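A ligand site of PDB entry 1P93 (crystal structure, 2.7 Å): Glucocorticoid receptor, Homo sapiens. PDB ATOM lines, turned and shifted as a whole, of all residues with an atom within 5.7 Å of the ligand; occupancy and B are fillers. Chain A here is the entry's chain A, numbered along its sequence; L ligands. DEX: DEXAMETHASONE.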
ATOM      1  N   MET A  63     -16.308   6.168  -2.633  1.00  0.00           N
ATOM      2  CA  MET A  63     -16.465   4.741  -2.824  1.00  0.00           C
ATOM      3  C   MET A  63     -17.653   4.542  -3.723  1.00  0.00           C
ATOM      4  O   MET A  63     -17.564   3.855  -4.747  1.00  0.00           O
ATOM      5  CB  MET A  63     -16.758   4.054  -1.497  1.00  0.00           C
ATOM      6  CG  MET A  63     -15.793   4.441  -0.398  1.00  0.00           C
ATOM      7  SD  MET A  63     -14.115   3.955  -0.814  1.00  0.00           S
ATOM      8  CE  MET A  63     -14.205   2.213  -0.317  1.00  0.00           C
ATOM      9  N   LEU A  66     -16.839   5.320  -7.059  1.00  0.00           N
ATOM     10  CA  LEU A  66     -16.000   4.372  -7.783  1.00  0.00           C
ATOM     11  C   LEU A  66     -16.910   3.290  -8.351  1.00  0.00           C
ATOM     12  O   LEU A  66     -16.826   2.946  -9.525  1.00  0.00           O
ATOM     13  CB  LEU A  66     -15.021   3.712  -6.835  1.00  0.00           C
ATOM     14  CG  LEU A  66     -14.325   4.683  -5.912  1.00  0.00           C
ATOM     15  CD1 LEU A  66     -13.381   3.908  -5.014  1.00  0.00           C
ATOM     16  CD2 LEU A  66     -13.587   5.713  -6.737  1.00  0.00           C
ATOM     17  N   ASN A  67     -17.782   2.772  -7.500  1.00  0.00           N
ATOM     18  CA  ASN A  67     -18.718   1.709  -7.878  1.00  0.00           C
ATOM     19  C   ASN A  67     -19.511   2.029  -9.134  1.00  0.00           C
ATOM     20  O   ASN A  67     -19.598   1.203 -10.034  1.00  0.00           O
ATOM     21  CB  ASN A  67     -19.676   1.448  -6.735  1.00  0.00           C
ATOM     22  CG  ASN A  67     -18.986   0.882  -5.529  1.00  0.00           C
ATOM     23  OD1 ASN A  67     -18.322  -0.151  -5.609  1.00  0.00           O
ATOM     24  ND2 ASN A  67     -19.130   1.553  -4.397  1.00  0.00           N
ATOM     25  N   MET A  68     -20.109   3.204  -9.188  1.00  0.00           N
ATOM     26  CA  MET A  68     -20.884   3.590 -10.355  1.00  0.00           C
ATOM     27  C   MET A  68     -19.984   3.452 -11.538  1.00  0.00           C
ATOM     28  O   MET A  68     -20.373   2.904 -12.571  1.00  0.00           O
ATOM     29  CB  MET A  68     -21.359   5.038 -10.249  1.00  0.00           C
ATOM     30  CG  MET A  68     -22.764   5.204  -9.678  1.00  0.00           C
ATOM     31  SD  MET A  68     -23.191   3.928  -8.486  1.00  0.00           S
ATOM     32  CE  MET A  68     -24.673   3.239  -9.223  1.00  0.00           C
ATOM     33  N   LEU A  69     -18.776   3.954 -11.381  1.00  0.00           N
ATOM     34  CA  LEU A  69     -17.763   3.896 -12.418  1.00  0.00           C
ATOM     35  C   LEU A  69     -17.337   2.460 -12.707  1.00  0.00           C
ATOM     36  O   LEU A  69     -17.101   2.084 -13.852  1.00  0.00           O
ATOM     37  CB  LEU A  69     -16.554   4.697 -11.978  1.00  0.00           C
ATOM     38  CG  LEU A  69     -15.278   4.351 -12.746  1.00  0.00           C
ATOM     39  CD1 LEU A  69     -15.406   4.880 -14.163  1.00  0.00           C
ATOM     40  CD2 LEU A  69     -14.067   4.940 -12.026  1.00  0.00           C
ATOM     41  N   GLY A  70     -17.229   1.665 -11.647  1.00  0.00           N
ATOM     42  CA  GLY A  70     -16.836   0.282 -11.819  1.00  0.00           C
ATOM     43  C   GLY A  70     -17.673  -0.392 -12.886  1.00  0.00           C
ATOM     44  O   GLY A  70     -17.138  -0.815 -13.907  1.00  0.00           O
ATOM     45  N   GLY A  71     -18.972  -0.454 -12.648  1.00  0.00           N
ATOM     46  CA  GLY A  71     -19.905  -1.075 -13.575  1.00  0.00           C
ATOM     47  C   GLY A  71     -19.691  -0.714 -15.026  1.00  0.00           C
ATOM     48  O   GLY A  71     -19.891  -1.551 -15.897  1.00  0.00           O
ATOM     49  N   GLN A  73     -16.747   0.315 -16.444  1.00  0.00           N
ATOM     50  CA  GLN A  73     -15.482  -0.275 -16.846  1.00  0.00           C
ATOM     51  C   GLN A  73     -15.749  -1.735 -17.140  1.00  0.00           C
ATOM     52  O   GLN A  73     -15.293  -2.296 -18.130  1.00  0.00           O
ATOM     53  CB  GLN A  73     -14.470  -0.184 -15.720  1.00  0.00           C
ATOM     54  CG  GLN A  73     -14.408   1.155 -15.053  1.00  0.00           C
ATOM     55  CD  GLN A  73     -13.009   1.475 -14.620  1.00  0.00           C
ATOM     56  OE1 GLN A  73     -12.751   2.527 -14.038  1.00  0.00           O
ATOM     57  NE2 GLN A  73     -12.073   0.572 -14.901  1.00  0.00           N
ATOM     58  N   TRP A 103     -13.560 -10.289 -12.983  1.00  0.00           N
ATOM     59  CA  TRP A 103     -13.850  -8.904 -13.282  1.00  0.00           C
ATOM     60  C   TRP A 103     -13.033  -8.060 -12.320  1.00  0.00           C
ATOM     61  O   TRP A 103     -12.397  -7.100 -12.717  1.00  0.00           O
ATOM     62  CB  TRP A 103     -15.350  -8.623 -13.124  1.00  0.00           C
ATOM     63  CG  TRP A 103     -15.826  -8.616 -11.750  1.00  0.00           C
ATOM     64  CD1 TRP A 103     -16.163  -9.692 -10.988  1.00  0.00           C
ATOM     65  CD2 TRP A 103     -15.989  -7.462 -10.917  1.00  0.00           C
ATOM     66  NE1 TRP A 103     -16.532  -9.279  -9.724  1.00  0.00           N
ATOM     67  CE2 TRP A 103     -16.442  -7.911  -9.665  1.00  0.00           C
ATOM     68  CE3 TRP A 103     -15.810  -6.090 -11.127  1.00  0.00           C
ATOM     69  CZ2 TRP A 103     -16.711  -7.037  -8.619  1.00  0.00           C
ATOM     70  CZ3 TRP A 103     -16.067  -5.232 -10.090  1.00  0.00           C
ATOM     71  CH2 TRP A 103     -16.508  -5.696  -8.848  1.00  0.00           C
ATOM     72  N   MET A 104     -13.039  -8.453 -11.055  1.00  0.00           N
ATOM     73  CA  MET A 104     -12.274  -7.742 -10.024  1.00  0.00           C
ATOM     74  C   MET A 104     -10.808  -7.702 -10.453  1.00  0.00           C
ATOM     75  O   MET A 104     -10.231  -6.632 -10.604  1.00  0.00           O
ATOM     76  CB  MET A 104     -12.391  -8.484  -8.684  1.00  0.00           C
ATOM     77  CG  MET A 104     -11.638  -7.830  -7.547  1.00  0.00           C
ATOM     78  SD  MET A 104     -12.018  -6.087  -7.490  1.00  0.00           S
ATOM     79  CE  MET A 104     -13.669  -6.099  -6.902  1.00  0.00           C
ATOM     80  N   MET A 107     -10.154  -5.393 -13.120  1.00  0.00           N
ATOM     81  CA  MET A 107     -10.402  -4.020 -12.693  1.00  0.00           C
ATOM     82  C   MET A 107      -9.242  -3.456 -11.907  1.00  0.00           C
ATOM     83  O   MET A 107      -8.901  -2.266 -12.018  1.00  0.00           O
ATOM     84  CB  MET A 107     -11.684  -3.957 -11.855  1.00  0.00           C
ATOM     85  CG  MET A 107     -12.968  -4.171 -12.658  1.00  0.00           C
ATOM     86  SD  MET A 107     -13.336  -2.825 -13.821  1.00  0.00           S
ATOM     87  CE  MET A 107     -12.114  -3.148 -15.166  1.00  0.00           C
ATOM     88  N   ALA A 108      -8.615  -4.319 -11.112  1.00  0.00           N
ATOM     89  CA  ALA A 108      -7.493  -3.922 -10.277  1.00  0.00           C
ATOM     90  C   ALA A 108      -6.177  -3.881 -11.026  1.00  0.00           C
ATOM     91  O   ALA A 108      -5.312  -3.057 -10.739  1.00  0.00           O
ATOM     92  CB  ALA A 108      -7.387  -4.873  -9.103  1.00  0.00           C
ATOM     93  N   LEU A 111      -6.060  -0.560 -13.211  1.00  0.00           N
ATOM     94  CA  LEU A 111      -5.854   0.591 -12.307  1.00  0.00           C
ATOM     95  C   LEU A 111      -4.419   0.705 -11.803  1.00  0.00           C
ATOM     96  O   LEU A 111      -3.874   1.813 -11.681  1.00  0.00           O
ATOM     97  CB  LEU A 111      -6.803   0.491 -11.098  1.00  0.00           C
ATOM     98  CG  LEU A 111      -6.353   1.129  -9.760  1.00  0.00           C
ATOM     99  CD1 LEU A 111      -6.244   2.630  -9.888  1.00  0.00           C
ATOM    100  CD2 LEU A 111      -7.339   0.774  -8.664  1.00  0.00           C
ATOM    101  N   ARG A 114      -2.603   2.389 -14.480  1.00  0.00           N
ATOM    102  CA  ARG A 114      -2.899   3.800 -14.444  1.00  0.00           C
ATOM    103  C   ARG A 114      -2.121   4.557 -13.371  1.00  0.00           C
ATOM    104  O   ARG A 114      -1.553   5.606 -13.641  1.00  0.00           O
ATOM    105  CB  ARG A 114      -4.391   3.998 -14.266  1.00  0.00           C
ATOM    106  CG  ARG A 114      -5.166   3.340 -15.382  1.00  0.00           C
ATOM    107  CD  ARG A 114      -6.509   4.005 -15.572  1.00  0.00           C
ATOM    108  NE  ARG A 114      -7.389   3.776 -14.444  1.00  0.00           N
ATOM    109  CZ  ARG A 114      -8.065   2.645 -14.238  1.00  0.00           C
ATOM    110  NH1 ARG A 114      -7.936   1.648 -15.102  1.00  0.00           N
ATOM    111  NH2 ARG A 114      -8.848   2.515 -13.189  1.00  0.00           N
ATOM    112  N   CYS A 125      -4.887   6.053  -8.966  1.00  0.00           N
ATOM    113  CA  CYS A 125      -5.535   6.721 -10.060  1.00  0.00           C
ATOM    114  C   CYS A 125      -6.717   5.904 -10.581  1.00  0.00           C
ATOM    115  O   CYS A 125      -6.549   4.956 -11.344  1.00  0.00           O
ATOM    116  CB  CYS A 125      -4.519   6.976 -11.160  1.00  0.00           C
ATOM    117  SG  CYS A 125      -5.246   6.782 -12.775  1.00  0.00           S
ATOM    118  N   PHE A 126      -7.921   6.277 -10.162  1.00  0.00           N
ATOM    119  CA  PHE A 126      -9.121   5.575 -10.587  1.00  0.00           C
ATOM    120  C   PHE A 126      -9.670   6.096 -11.880  1.00  0.00           C
ATOM    121  O   PHE A 126     -10.215   5.347 -12.686  1.00  0.00           O
ATOM    122  CB  PHE A 126     -10.175   5.696  -9.487  1.00  0.00           C
ATOM    123  CG  PHE A 126      -9.877   4.842  -8.310  1.00  0.00           C
ATOM    124  CD1 PHE A 126     -10.141   3.480  -8.342  1.00  0.00           C
ATOM    125  CD2 PHE A 126      -9.249   5.363  -7.198  1.00  0.00           C
ATOM    126  CE1 PHE A 126      -9.788   2.667  -7.293  1.00  0.00           C
ATOM    127  CE2 PHE A 126      -8.898   4.553  -6.135  1.00  0.00           C
ATOM    128  CZ  PHE A 126      -9.160   3.193  -6.190  1.00  0.00           C
ATOM    129  N   GLN A 145      -7.925  -0.043   2.651  1.00  0.00           N
ATOM    130  CA  GLN A 145      -8.234  -0.912   1.523  1.00  0.00           C
ATOM    131  C   GLN A 145      -7.428  -0.576   0.284  1.00  0.00           C
ATOM    132  O   GLN A 145      -7.213  -1.434  -0.574  1.00  0.00           O
ATOM    133  CB  GLN A 145      -9.723  -0.815   1.199  1.00  0.00           C
ATOM    134  CG  GLN A 145     -10.189   0.567   0.827  1.00  0.00           C
ATOM    135  CD  GLN A 145     -11.684   0.694   0.853  1.00  0.00           C
ATOM    136  OE1 GLN A 145     -12.398  -0.084   0.206  1.00  0.00           O
ATOM    137  NE2 GLN A 145     -12.185   1.667   1.594  1.00  0.00           N
ATOM    138  N   MET A 149      -4.526  -2.185  -3.589  1.00  0.00           N
ATOM    139  CA  MET A 149      -4.455  -1.664  -4.950  1.00  0.00           C
ATOM    140  C   MET A 149      -3.080  -1.045  -5.204  1.00  0.00           C
ATOM    141  O   MET A 149      -2.566  -1.086  -6.327  1.00  0.00           O
ATOM    142  CB  MET A 149      -5.537  -0.596  -5.134  1.00  0.00           C
ATOM    143  CG  MET A 149      -6.857  -0.930  -4.487  1.00  0.00           C
ATOM    144  SD  MET A 149      -8.064   0.356  -4.781  1.00  0.00           S
ATOM    145  CE  MET A 149      -9.306  -0.544  -5.638  1.00  0.00           C
ATOM    146  N   LEU A 235     -10.122  -7.859  -1.789  1.00  0.00           N
ATOM    147  CA  LEU A 235     -10.989  -6.857  -2.367  1.00  0.00           C
ATOM    148  C   LEU A 235     -12.440  -7.277  -2.332  1.00  0.00           C
ATOM    149  O   LEU A 235     -13.337  -6.453  -2.218  1.00  0.00           O
ATOM    150  CB  LEU A 235     -10.583  -6.611  -3.818  1.00  0.00           C
ATOM    151  CG  LEU A 235      -9.100  -6.309  -3.999  1.00  0.00           C
ATOM    152  CD1 LEU A 235      -8.859  -6.105  -5.477  1.00  0.00           C
ATOM    153  CD2 LEU A 235      -8.696  -5.060  -3.186  1.00  0.00           C
ATOM    154  N   TYR A 238     -13.732  -7.036   1.207  1.00  0.00           N
ATOM    155  CA  TYR A 238     -14.075  -5.676   1.578  1.00  0.00           C
ATOM    156  C   TYR A 238     -15.300  -5.211   0.826  1.00  0.00           C
ATOM    157  O   TYR A 238     -16.153  -4.499   1.353  1.00  0.00           O
ATOM    158  CB  TYR A 238     -12.918  -4.744   1.249  1.00  0.00           C
ATOM    159  CG  TYR A 238     -12.845  -3.629   2.236  1.00  0.00           C
ATOM    160  CD1 TYR A 238     -13.950  -2.838   2.505  1.00  0.00           C
ATOM    161  CD2 TYR A 238     -11.667  -3.379   2.919  1.00  0.00           C
ATOM    162  CE1 TYR A 238     -13.894  -1.823   3.440  1.00  0.00           C
ATOM    163  CE2 TYR A 238     -11.592  -2.354   3.861  1.00  0.00           C
ATOM    164  CZ  TYR A 238     -12.705  -1.575   4.111  1.00  0.00           C
ATOM    165  OH  TYR A 238     -12.620  -0.534   5.028  1.00  0.00           O
ATOM    166  N   CYS A 239     -15.384  -5.632  -0.434  1.00  0.00           N
ATOM    167  CA  CYS A 239     -16.486  -5.301  -1.305  1.00  0.00           C
ATOM    168  C   CYS A 239     -17.786  -5.972  -0.895  1.00  0.00           C
ATOM    169  O   CYS A 239     -18.858  -5.394  -1.091  1.00  0.00           O
ATOM    170  CB  CYS A 239     -16.176  -5.708  -2.743  1.00  0.00           C
ATOM    171  SG  CYS A 239     -17.651  -5.777  -3.762  1.00  0.00           S
ATOM    172  N   PHE A 240     -17.714  -7.175  -0.329  1.00  0.00           N
ATOM    173  CA  PHE A 240     -18.944  -7.828   0.069  1.00  0.00           C
ATOM    174  C   PHE A 240     -19.571  -7.256   1.325  1.00  0.00           C
ATOM    175  O   PHE A 240     -20.787  -7.126   1.390  1.00  0.00           O
ATOM    176  CB  PHE A 240     -18.785  -9.363   0.143  1.00  0.00           C
ATOM    177  CG  PHE A 240     -18.049  -9.904   1.377  1.00  0.00           C
ATOM    178  CD1 PHE A 240     -18.482  -9.583   2.677  1.00  0.00           C
ATOM    179  CD2 PHE A 240     -17.011 -10.818   1.231  1.00  0.00           C
ATOM    180  CE1 PHE A 240     -17.884 -10.177   3.795  1.00  0.00           C
ATOM    181  CE2 PHE A 240     -16.401 -11.420   2.344  1.00  0.00           C
ATOM    182  CZ  PHE A 240     -16.844 -11.089   3.627  1.00  0.00           C
ATOM    183  N   THR A 242     -19.347  -4.161   2.509  1.00  0.00           N
ATOM    184  CA  THR A 242     -19.870  -2.868   2.057  1.00  0.00           C
ATOM    185  C   THR A 242     -21.106  -2.990   1.159  1.00  0.00           C
ATOM    186  O   THR A 242     -21.968  -2.103   1.123  1.00  0.00           O
ATOM    187  CB  THR A 242     -18.794  -2.123   1.290  1.00  0.00           C
ATOM    188  OG1 THR A 242     -18.296  -2.964   0.243  1.00  0.00           O
ATOM    189  CG2 THR A 242     -17.646  -1.751   2.227  1.00  0.00           C
ATOM    190  N   PHE A 243     -21.148  -4.086   0.432  1.00  0.00           N
ATOM    191  CA  PHE A 243     -22.257  -4.378  -0.454  1.00  0.00           C
ATOM    192  C   PHE A 243     -23.426  -4.861   0.406  1.00  0.00           C
ATOM    193  O   PHE A 243     -24.596  -4.688   0.037  1.00  0.00           O
ATOM    194  CB  PHE A 243     -21.829  -5.466  -1.446  1.00  0.00           C
ATOM    195  CG  PHE A 243     -22.929  -5.967  -2.299  1.00  0.00           C
ATOM    196  CD1 PHE A 243     -23.579  -5.120  -3.186  1.00  0.00           C
ATOM    197  CD2 PHE A 243     -23.346  -7.288  -2.223  1.00  0.00           C
ATOM    198  CE1 PHE A 243     -24.617  -5.580  -3.977  1.00  0.00           C
ATOM    199  CE2 PHE A 243     -24.374  -7.753  -3.005  1.00  0.00           C
ATOM    200  CZ  PHE A 243     -25.016  -6.888  -3.882  1.00  0.00           C
ATOM    201  N   ILE A 250     -23.112   2.876   1.254  1.00  0.00           N
ATOM    202  CA  ILE A 250     -22.405   2.817  -0.022  1.00  0.00           C
ATOM    203  C   ILE A 250     -23.315   2.145  -1.052  1.00  0.00           C
ATOM    204  O   ILE A 250     -23.994   1.165  -0.728  1.00  0.00           O
ATOM    205  CB  ILE A 250     -21.050   2.046   0.149  1.00  0.00           C
ATOM    206  CG1 ILE A 250     -20.062   2.932   0.913  1.00  0.00           C
ATOM    207  CG2 ILE A 250     -20.464   1.651  -1.208  1.00  0.00           C
ATOM    208  CD1 ILE A 250     -18.620   2.456   0.844  1.00  0.00           C
ATOM    209  N   PHE A 252     -23.928   0.442  -5.084  1.00  0.00           N
ATOM    210  CA  PHE A 252     -23.322  -0.180  -6.265  1.00  0.00           C
ATOM    211  C   PHE A 252     -24.219  -0.050  -7.488  1.00  0.00           C
ATOM    212  O   PHE A 252     -25.439  -0.016  -7.366  1.00  0.00           O
ATOM    213  CB  PHE A 252     -23.077  -1.677  -6.026  1.00  0.00           C
ATOM    214  CG  PHE A 252     -22.083  -1.971  -4.954  1.00  0.00           C
ATOM    215  CD1 PHE A 252     -22.275  -1.534  -3.650  1.00  0.00           C
ATOM    216  CD2 PHE A 252     -20.941  -2.712  -5.238  1.00  0.00           C
ATOM    217  CE1 PHE A 252     -21.367  -1.826  -2.660  1.00  0.00           C
ATOM    218  CE2 PHE A 252     -20.032  -3.009  -4.239  1.00  0.00           C
ATOM    219  CZ  PHE A 252     -20.235  -2.567  -2.945  1.00  0.00           C
ATOM    220  N   LEU A 256     -22.778  -4.555 -11.066  1.00  0.00           N
ATOM    221  CA  LEU A 256     -22.099  -5.305 -10.022  1.00  0.00           C
ATOM    222  C   LEU A 256     -23.074  -6.038  -9.118  1.00  0.00           C
ATOM    223  O   LEU A 256     -22.670  -6.884  -8.325  1.00  0.00           O
ATOM    224  CB  LEU A 256     -21.252  -4.353  -9.206  1.00  0.00           C
ATOM    225  CG  LEU A 256     -20.732  -3.224 -10.087  1.00  0.00           C
ATOM    226  CD1 LEU A 256     -19.766  -2.352  -9.285  1.00  0.00           C
ATOM    227  CD2 LEU A 256     -20.072  -3.833 -11.331  1.00  0.00           C
HETATM  228  C1  DEX L   1     -13.665   0.927  -9.778  1.00  0.00           C
HETATM  229  C2  DEX L   1     -12.812   1.581 -10.698  1.00  0.00           C
HETATM  230  C3  DEX L   1     -11.484   0.935 -11.052  1.00  0.00           C
HETATM  231  C4  DEX L   1     -11.142  -0.417 -10.378  1.00  0.00           C
HETATM  232  C5  DEX L   1     -11.984  -1.073  -9.471  1.00  0.00           C
HETATM  233  C6  DEX L   1     -11.586  -2.502  -8.775  1.00  0.00           C
HETATM  234  C7  DEX L   1     -11.770  -2.417  -7.232  1.00  0.00           C
HETATM  235  C8  DEX L   1     -13.217  -1.868  -6.751  1.00  0.00           C
HETATM  236  C9  DEX L   1     -13.560  -0.429  -7.394  1.00  0.00           C
HETATM  237  C10 DEX L   1     -13.404  -0.472  -9.028  1.00  0.00           C
HETATM  238  C11 DEX L   1     -14.973   0.158  -6.888  1.00  0.00           C
HETATM  239  C12 DEX L   1     -15.075   0.129  -5.335  1.00  0.00           C
HETATM  240  C13 DEX L   1     -14.697  -1.245  -4.580  1.00  0.00           C
HETATM  241  C14 DEX L   1     -13.327  -1.762  -5.148  1.00  0.00           C
HETATM  242  C15 DEX L   1     -13.073  -3.069  -4.280  1.00  0.00           C
HETATM  243  C16 DEX L   1     -13.264  -2.515  -2.880  1.00  0.00           C
HETATM  244  C17 DEX L   1     -14.291  -1.313  -3.037  1.00  0.00           C
HETATM  245  C18 DEX L   1     -15.969  -2.236  -4.844  1.00  0.00           C
HETATM  246  C19 DEX L   1     -14.490  -1.478  -9.644  1.00  0.00           C
HETATM  247  C20 DEX L   1     -15.431  -1.207  -1.971  1.00  0.00           C
HETATM  248  C21 DEX L   1     -16.425  -0.086  -2.049  1.00  0.00           C
HETATM  249  C22 DEX L   1     -11.891  -2.066  -2.259  1.00  0.00           C
HETATM  250  F1  DEX L   1     -12.596   0.442  -7.006  1.00  0.00           F
HETATM  251  O1  DEX L   1     -10.632   1.435 -11.880  1.00  0.00           O
HETATM  252  O2  DEX L   1     -16.112  -0.395  -7.384  1.00  0.00           O
HETATM  253  O3  DEX L   1     -13.716  -0.125  -2.581  1.00  0.00           O
HETATM  254  O4  DEX L   1     -15.484  -2.100  -1.056  1.00  0.00           O
HETATM  255  O5  DEX L   1     -17.330  -0.190  -1.031  1.00  0.00           O
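NH2 of Arg 114 is in hydrogen-bond range of O of Phe 126 (3.2 Å). NE of Arg 114 sits at hydrogen-bond distance from O of Cys 125, at 3.4 Å. The side-chain amide nitrogen (ND2) of Asn 67 is in hydrogen-bond range of the backbone carbonyl oxygen (O) of Met 63 (2.8 Å). O of Tyr 238 sits at hydrogen-bond distance from OG1 of Thr 242 (2.9 Å). The side-chain hydroxyl of Thr 242 sits at hydrogen-bond distance from the backbone carbonyl oxygen of Cys 239, at 2.8 Å. The side-chain amide nitrogen (NE2) of Gln 73 sits close to the side-chain sulfur (SD) of Met 107 (3.8 Å).
An oxygen (O1) of the ligand sits at hydrogen-bond distance from the guanidinium group (NH2) of Arg 114 (2.5 Å). The side-chain amide oxygen (OD1) of Asn 67 is in hydrogen-bond range of an oxygen (O2) of the ligand, 2.8 Å away. OE1 of Gln 145 sits at hydrogen-bond distance from O3 of the ligand (3.1 Å). The side-chain hydroxyl (OG1) of Thr 242 sits at hydrogen-bond distance from an oxygen (O5) of the ligand, at 3.2 Å. The side-chain amide oxygen (OE1) of Gln 73 lies close to an oxygen (O1) of the ligand (3.2 Å).
The backbone carbonyl oxygen (O) of Tyr 238 sits close to an oxygen (O4) of the ligand, at 3.5 Å. Residues that only touch the ligand: Met 63, Met 107, Cys 239, Met 149, Ile 250, Leu 66, Phe 126, Gly 70, Met 104, Leu 69 and Leu 235. Hydrophobic or aromatic side chains that line the ligand: Met 63, Leu 66, Leu 69, Met 104, Met 107, Phe 126, Met 149, Tyr 238 and Ile 250. Along chain A the residues within 4 Å of the ligand span positions 63 to 250.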
